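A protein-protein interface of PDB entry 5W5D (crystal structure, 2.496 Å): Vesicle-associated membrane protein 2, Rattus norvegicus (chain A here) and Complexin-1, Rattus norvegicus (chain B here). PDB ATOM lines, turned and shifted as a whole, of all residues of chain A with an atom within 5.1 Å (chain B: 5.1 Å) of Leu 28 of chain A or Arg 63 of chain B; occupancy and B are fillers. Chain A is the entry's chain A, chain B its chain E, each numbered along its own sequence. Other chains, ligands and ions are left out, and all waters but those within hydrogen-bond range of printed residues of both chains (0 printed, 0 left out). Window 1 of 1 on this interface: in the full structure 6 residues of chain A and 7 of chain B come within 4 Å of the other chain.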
ATOM      1  N   ASN A  23     -35.178 -23.298  26.847  1.00  0.00           N
ATOM      2  CA  ASN A  23     -34.242 -23.443  27.962  1.00  0.00           C
ATOM      3  C   ASN A  23     -32.844 -22.987  27.581  1.00  0.00           C
ATOM      4  O   ASN A  23     -32.136 -22.391  28.400  1.00  0.00           O
ATOM      5  CB  ASN A  23     -34.199 -24.890  28.451  1.00  0.00           C
ATOM      6  CG  ASN A  23     -35.525 -25.362  28.993  1.00  0.00           C
ATOM      7  OD1 ASN A  23     -36.357 -24.563  29.425  1.00  0.00           O
ATOM      8  ND2 ASN A  23     -35.728 -26.676  28.986  1.00  0.00           N
ATOM      9  N   VAL A  24     -32.420 -23.265  26.345  1.00  0.00           N
ATOM     10  CA  VAL A  24     -31.088 -22.860  25.913  1.00  0.00           C
ATOM     11  C   VAL A  24     -30.991 -21.344  25.853  1.00  0.00           C
ATOM     12  O   VAL A  24     -29.970 -20.759  26.242  1.00  0.00           O
ATOM     13  CB  VAL A  24     -30.730 -23.507  24.562  1.00  0.00           C
ATOM     14  CG1 VAL A  24     -29.482 -22.862  23.978  1.00  0.00           C
ATOM     15  CG2 VAL A  24     -30.505 -24.996  24.731  1.00  0.00           C
ATOM     16  N   ASP A  25     -32.048 -20.675  25.384  1.00  0.00           N
ATOM     17  CA  ASP A  25     -32.029 -19.215  25.448  1.00  0.00           C
ATOM     18  C   ASP A  25     -31.880 -18.736  26.890  1.00  0.00           C
ATOM     19  O   ASP A  25     -31.025 -17.890  27.195  1.00  0.00           O
ATOM     20  CB  ASP A  25     -33.290 -18.634  24.807  1.00  0.00           C
ATOM     21  CG  ASP A  25     -33.212 -17.128  24.642  1.00  0.00           C
ATOM     22  OD1 ASP A  25     -32.184 -16.640  24.121  1.00  0.00           O
ATOM     23  OD2 ASP A  25     -34.176 -16.436  25.031  1.00  0.00           O
ATOM     24  N   LYS A  26     -32.684 -19.301  27.800  1.00  0.00           N
ATOM     25  CA  LYS A  26     -32.621 -18.887  29.200  1.00  0.00           C
ATOM     26  C   LYS A  26     -31.225 -19.087  29.788  1.00  0.00           C
ATOM     27  O   LYS A  26     -30.708 -18.212  30.493  1.00  0.00           O
ATOM     28  CB  LYS A  26     -33.660 -19.653  30.012  1.00  0.00           C
ATOM     29  CG  LYS A  26     -35.090 -19.226  29.762  1.00  0.00           C
ATOM     30  CD  LYS A  26     -36.067 -20.128  30.513  1.00  0.00           C
ATOM     31  CE  LYS A  26     -37.513 -19.746  30.218  1.00  0.00           C
ATOM     32  NZ  LYS A  26     -38.481 -20.738  30.763  1.00  0.00           N
ATOM     33  N   VAL A  27     -30.597 -20.234  29.510  1.00  0.00           N
ATOM     34  CA  VAL A  27     -29.274 -20.513  30.052  1.00  0.00           C
ATOM     35  C   VAL A  27     -28.201 -19.679  29.370  1.00  0.00           C
ATOM     36  O   VAL A  27     -27.109 -19.510  29.925  1.00  0.00           O
ATOM     37  CB  VAL A  27     -28.941 -22.015  29.941  1.00  0.00           C
ATOM     38  CG1 VAL A  27     -28.376 -22.340  28.567  1.00  0.00           C
ATOM     39  CG2 VAL A  27     -27.967 -22.440  31.042  1.00  0.00           C
ATOM     40  N   LEU A  28     -28.471 -19.158  28.171  1.00  0.00           N
ATOM     41  CA  LEU A  28     -27.529 -18.217  27.575  1.00  0.00           C
ATOM     42  C   LEU A  28     -27.619 -16.858  28.259  1.00  0.00           C
ATOM     43  O   LEU A  28     -26.592 -16.205  28.493  1.00  0.00           O
ATOM     44  CB  LEU A  28     -27.777 -18.110  26.073  1.00  0.00           C
ATOM     45  CG  LEU A  28     -27.260 -19.345  25.331  1.00  0.00           C
ATOM     46  CD1 LEU A  28     -27.569 -19.274  23.846  1.00  0.00           C
ATOM     47  CD2 LEU A  28     -25.769 -19.522  25.569  1.00  0.00           C
ATOM     48  N   GLU A  29     -28.837 -16.420  28.600  1.00  0.00           N
ATOM     49  CA  GLU A  29     -28.965 -15.283  29.507  1.00  0.00           C
ATOM     50  C   GLU A  29     -28.196 -15.534  30.799  1.00  0.00           C
ATOM     51  O   GLU A  29     -27.474 -14.654  31.289  1.00  0.00           O
ATOM     52  CB  GLU A  29     -30.437 -15.014  29.817  1.00  0.00           C
ATOM     53  CG  GLU A  29     -31.270 -14.590  28.624  1.00  0.00           C
ATOM     54  CD  GLU A  29     -32.692 -14.229  29.009  1.00  0.00           C
ATOM     55  OE1 GLU A  29     -33.035 -14.368  30.205  1.00  0.00           O
ATOM     56  OE2 GLU A  29     -33.464 -13.804  28.120  1.00  0.00           O
ATOM     57  N   ARG A  30     -28.334 -16.740  31.355  1.00  0.00           N
ATOM     58  CA  ARG A  30     -27.622 -17.092  32.580  1.00  0.00           C
ATOM     59  C   ARG A  30     -26.113 -16.980  32.397  1.00  0.00           C
ATOM     60  O   ARG A  30     -25.409 -16.480  33.284  1.00  0.00           O
ATOM     61  CB  ARG A  30     -28.010 -18.506  33.010  1.00  0.00           C
ATOM     62  CG  ARG A  30     -27.482 -18.942  34.366  1.00  0.00           C
ATOM     63  CD  ARG A  30     -27.984 -20.340  34.691  1.00  0.00           C
ATOM     64  NE  ARG A  30     -27.826 -20.697  36.097  1.00  0.00           N
ATOM     65  CZ  ARG A  30     -26.798 -21.386  36.582  1.00  0.00           C
ATOM     66  NH1 ARG A  30     -25.825 -21.784  35.775  1.00  0.00           N
ATOM     67  NH2 ARG A  30     -26.741 -21.674  37.877  1.00  0.00           N
ATOM     68  N   ASP A  31     -25.597 -17.438  31.254  1.00  0.00           N
ATOM     69  CA  ASP A  31     -24.162 -17.335  31.004  1.00  0.00           C
ATOM     70  C   ASP A  31     -23.731 -15.879  30.913  1.00  0.00           C
ATOM     71  O   ASP A  31     -22.668 -15.510  31.422  1.00  0.00           O
ATOM     72  CB  ASP A  31     -23.798 -18.089  29.723  1.00  0.00           C
ATOM     73  CG  ASP A  31     -22.293 -18.203  29.503  1.00  0.00           C
ATOM     74  OD1 ASP A  31     -21.587 -17.174  29.499  1.00  0.00           O
ATOM     75  OD2 ASP A  31     -21.818 -19.340  29.296  1.00  0.00           O
ATOM     76  N   GLN A  32     -24.538 -15.040  30.263  1.00  0.00           N
ATOM     77  CA  GLN A  32     -24.227 -13.617  30.195  1.00  0.00           C
ATOM     78  C   GLN A  32     -24.118 -13.017  31.593  1.00  0.00           C
ATOM     79  O   GLN A  32     -23.083 -12.442  31.964  1.00  0.00           O
ATOM     80  CB  GLN A  32     -25.300 -12.899  29.373  1.00  0.00           C
ATOM     81  CG  GLN A  32     -25.076 -11.410  29.168  1.00  0.00           C
ATOM     82  CD  GLN A  32     -26.267 -10.738  28.510  1.00  0.00           C
ATOM     83  OE1 GLN A  32     -27.318 -11.356  28.326  1.00  0.00           O
ATOM     84  NE2 GLN A  32     -26.111  -9.469  28.150  1.00  0.00           N
ATOM     85  N   SER A  35     -21.210 -14.324  33.595  1.00  0.00           N
ATOM     86  CA  SER A  35     -19.944 -13.821  33.079  1.00  0.00           C
ATOM     87  C   SER A  35     -19.706 -12.381  33.508  1.00  0.00           C
ATOM     88  O   SER A  35     -18.554 -11.984  33.724  1.00  0.00           O
ATOM     89  CB  SER A  35     -19.907 -13.941  31.557  1.00  0.00           C
ATOM     90  OG  SER A  35     -19.756 -15.292  31.162  1.00  0.00           O
ATOM     91  N   GLU B  56     -14.172 -12.192  26.872  1.00  0.00           N
ATOM     92  CA  GLU B  56     -15.626 -12.071  26.856  1.00  0.00           C
ATOM     93  C   GLU B  56     -16.154 -12.008  25.428  1.00  0.00           C
ATOM     94  O   GLU B  56     -17.087 -12.740  25.070  1.00  0.00           O
ATOM     95  CB  GLU B  56     -16.070 -10.840  27.648  1.00  0.00           C
ATOM     96  CG  GLU B  56     -17.552 -10.515  27.514  1.00  0.00           C
ATOM     97  CD  GLU B  56     -18.458 -11.663  27.943  1.00  0.00           C
ATOM     98  OE1 GLU B  56     -18.056 -12.462  28.818  1.00  0.00           O
ATOM     99  OE2 GLU B  56     -19.583 -11.762  27.406  1.00  0.00           O
ATOM    100  N   ARG B  59     -16.259 -15.266  23.802  1.00  0.00           N
ATOM    101  CA  ARG B  59     -17.317 -16.104  24.352  1.00  0.00           C
ATOM    102  C   ARG B  59     -18.672 -15.747  23.753  1.00  0.00           C
ATOM    103  O   ARG B  59     -19.453 -16.639  23.394  1.00  0.00           O
ATOM    104  CB  ARG B  59     -17.358 -15.993  25.876  1.00  0.00           C
ATOM    105  CG  ARG B  59     -18.313 -16.997  26.509  1.00  0.00           C
ATOM    106  CD  ARG B  59     -18.083 -17.182  27.998  1.00  0.00           C
ATOM    107  NE  ARG B  59     -18.978 -18.205  28.536  1.00  0.00           N
ATOM    108  CZ  ARG B  59     -18.736 -19.511  28.483  1.00  0.00           C
ATOM    109  NH1 ARG B  59     -17.619 -19.958  27.925  1.00  0.00           N
ATOM    110  NH2 ARG B  59     -19.608 -20.370  28.990  1.00  0.00           N
ATOM    111  N   GLU B  60     -18.958 -14.449  23.608  1.00  0.00           N
ATOM    112  CA  GLU B  60     -20.235 -14.065  23.017  1.00  0.00           C
ATOM    113  C   GLU B  60     -20.373 -14.623  21.610  1.00  0.00           C
ATOM    114  O   GLU B  60     -21.465 -15.057  21.223  1.00  0.00           O
ATOM    115  CB  GLU B  60     -20.393 -12.544  23.021  1.00  0.00           C
ATOM    116  CG  GLU B  60     -21.665 -12.036  22.345  1.00  0.00           C
ATOM    117  CD  GLU B  60     -22.942 -12.638  22.913  1.00  0.00           C
ATOM    118  OE1 GLU B  60     -22.972 -12.982  24.115  1.00  0.00           O
ATOM    119  OE2 GLU B  60     -23.926 -12.763  22.151  1.00  0.00           O
ATOM    120  N   VAL B  61     -19.273 -14.666  20.850  1.00  0.00           N
ATOM    121  CA  VAL B  61     -19.300 -15.340  19.556  1.00  0.00           C
ATOM    122  C   VAL B  61     -19.839 -16.753  19.725  1.00  0.00           C
ATOM    123  O   VAL B  61     -20.855 -17.124  19.119  1.00  0.00           O
ATOM    124  CB  VAL B  61     -17.901 -15.337  18.911  1.00  0.00           C
ATOM    125  CG1 VAL B  61     -17.791 -16.440  17.863  1.00  0.00           C
ATOM    126  CG2 VAL B  61     -17.602 -13.985  18.291  1.00  0.00           C
ATOM    127  N   MET B  62     -19.204 -17.534  20.610  1.00  0.00           N
ATOM    128  CA  MET B  62     -19.684 -18.875  20.925  1.00  0.00           C
ATOM    129  C   MET B  62     -21.169 -18.855  21.260  1.00  0.00           C
ATOM    130  O   MET B  62     -21.946 -19.659  20.731  1.00  0.00           O
ATOM    131  CB  MET B  62     -18.865 -19.458  22.081  1.00  0.00           C
ATOM    132  CG  MET B  62     -19.265 -20.869  22.523  1.00  0.00           C
ATOM    133  SD  MET B  62     -20.431 -20.850  23.897  1.00  0.00           S
ATOM    134  CE  MET B  62     -19.387 -20.201  25.192  1.00  0.00           C
ATOM    135  N   ARG B  63     -21.593 -17.900  22.096  1.00  0.00           N
ATOM    136  CA  ARG B  63     -23.001 -17.836  22.475  1.00  0.00           C
ATOM    137  C   ARG B  63     -23.876 -17.628  21.247  1.00  0.00           C
ATOM    138  O   ARG B  63     -24.858 -18.356  21.036  1.00  0.00           O
ATOM    139  CB  ARG B  63     -23.223 -16.729  23.506  1.00  0.00           C
ATOM    140  CG  ARG B  63     -22.857 -17.147  24.926  1.00  0.00           C
ATOM    141  CD  ARG B  63     -23.489 -16.243  25.977  1.00  0.00           C
ATOM    142  NE  ARG B  63     -22.738 -15.006  26.176  1.00  0.00           N
ATOM    143  CZ  ARG B  63     -21.685 -14.889  26.980  1.00  0.00           C
ATOM    144  NH1 ARG B  63     -21.250 -15.936  27.660  1.00  0.00           N
ATOM    145  NH2 ARG B  63     -21.064 -13.725  27.101  1.00  0.00           N
ATOM    146  N   GLN B  64     -23.504 -16.668  20.396  1.00  0.00           N
ATOM    147  CA  GLN B  64     -24.246 -16.477  19.157  1.00  0.00           C
ATOM    148  C   GLN B  64     -24.192 -17.735  18.300  1.00  0.00           C
ATOM    149  O   GLN B  64     -25.203 -18.136  17.705  1.00  0.00           O
ATOM    150  CB  GLN B  64     -23.702 -15.269  18.400  1.00  0.00           C
ATOM    151  CG  GLN B  64     -24.667 -14.737  17.361  1.00  0.00           C
ATOM    152  CD  GLN B  64     -26.043 -14.493  17.936  1.00  0.00           C
ATOM    153  OE1 GLN B  64     -26.185 -13.921  19.019  1.00  0.00           O
ATOM    154  NE2 GLN B  64     -27.069 -14.934  17.219  1.00  0.00           N
ATOM    155  N   GLY B  65     -23.033 -18.400  18.276  1.00  0.00           N
ATOM    156  CA  GLY B  65     -22.934 -19.665  17.570  1.00  0.00           C
ATOM    157  C   GLY B  65     -24.003 -20.650  17.994  1.00  0.00           C
ATOM    158  O   GLY B  65     -24.566 -21.366  17.161  1.00  0.00           O
ATOM    159  N   ILE B  66     -24.316 -20.685  19.293  1.00  0.00           N
ATOM    160  CA  ILE B  66     -25.393 -21.550  19.764  1.00  0.00           C
ATOM    161  C   ILE B  66     -26.737 -21.033  19.264  1.00  0.00           C
ATOM    162  O   ILE B  66     -27.520 -21.780  18.660  1.00  0.00           O
ATOM    163  CB  ILE B  66     -25.370 -21.663  21.300  1.00  0.00           C
ATOM    164  CG1 ILE B  66     -24.087 -22.349  21.777  1.00  0.00           C
ATOM    165  CG2 ILE B  66     -26.600 -22.416  21.800  1.00  0.00           C
ATOM    166  CD1 ILE B  66     -23.928 -23.760  21.261  1.00  0.00           C
ATOM    167  N   ARG B  67     -27.003 -19.738  19.470  1.00  0.00           N
ATOM    168  CA  ARG B  67     -28.303 -19.174  19.113  1.00  0.00           C
ATOM    169  C   ARG B  67     -28.617 -19.414  17.643  1.00  0.00           C
ATOM    170  O   ARG B  67     -29.725 -19.839  17.292  1.00  0.00           O
ATOM    171  CB  ARG B  67     -28.333 -17.678  19.429  1.00  0.00           C
ATOM    172  CG  ARG B  67     -28.520 -17.363  20.898  1.00  0.00           C
ATOM    173  CD  ARG B  67     -28.664 -15.873  21.137  1.00  0.00           C
ATOM    174  NE  ARG B  67     -29.211 -15.596  22.461  1.00  0.00           N
ATOM    175  CZ  ARG B  67     -28.473 -15.350  23.538  1.00  0.00           C
ATOM    176  NH1 ARG B  67     -27.149 -15.342  23.449  1.00  0.00           N
ATOM    177  NH2 ARG B  67     -29.060 -15.110  24.704  1.00  0.00           N
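OD1 of Asp 25 of chain A lies within salt-bridge range of NH2 of Arg 67 of chain B (3.5 Å). NH2 of Arg 59 of chain B is in salt-bridge range of OD2 of Asp 31 of chain A. OD2 of Asp 31 of chain A is in salt-bridge range of NH1 of Arg 63 of chain B.
O of Asp 31 of chain A lies within hydrogen-bond range of OG of Ser 35 of chain A (2.9 Å). OE2 of Glu 56 of chain B is in salt-bridge range of NH2 of Arg 63 of chain B (2.5 Å). OE1 of Glu 60 of chain B is in salt-bridge range of NE of Arg 63 of chain B, 2.9 Å away.
Among the printed residues, merely in contact across the chains: Leu 28 of chain A with Arg 67 of chain B, Ser 35 of chain A with Glu 56 of chain B, Val 24 of chain A with Ile 66 of chain B, Leu 28 of chain A with Arg 63 of chain B, Ser 35 of chain A with Arg 63 of chain B, Leu 28 of chain A with Ile 66 of chain B and Ser 35 of chain A with Arg 59 of chain B.
Leu 28 of chain A touches just these residues of chain B: Arg 63 (3.8 Å), Ile 66 (3.9 Å) and Arg 67 (3.5 Å). Arg 63 of chain B touches just these residues of chain A: Leu 28, Asp 31 and Ser 35. Of the printed residues of chain A, Ile 66 of chain B touches Val 24 and Leu 28. Printed residues of chain A within 4 Å of Arg 59 of chain B: Asp 31 and Ser 35. Gly 65 of chain B touches none of the printed residues of chain A. The nearest printed residue of chain B that does not touch Leu 28 of chain A is Met 62 of chain B (5.7 Å). The nearest residue of chain A that does not touch Arg 63 of chain B is Gln 32 of chain A (4.3 Å).
Of the 11 printed residues of chain A, 5 touch a printed residue of chain B. Hydrophobic or aromatic side chains of chain A that line the printed part of chain B: Val 24 and Leu 28. Of the 10 printed residues of chain B, 5 touch a printed residue of chain A.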
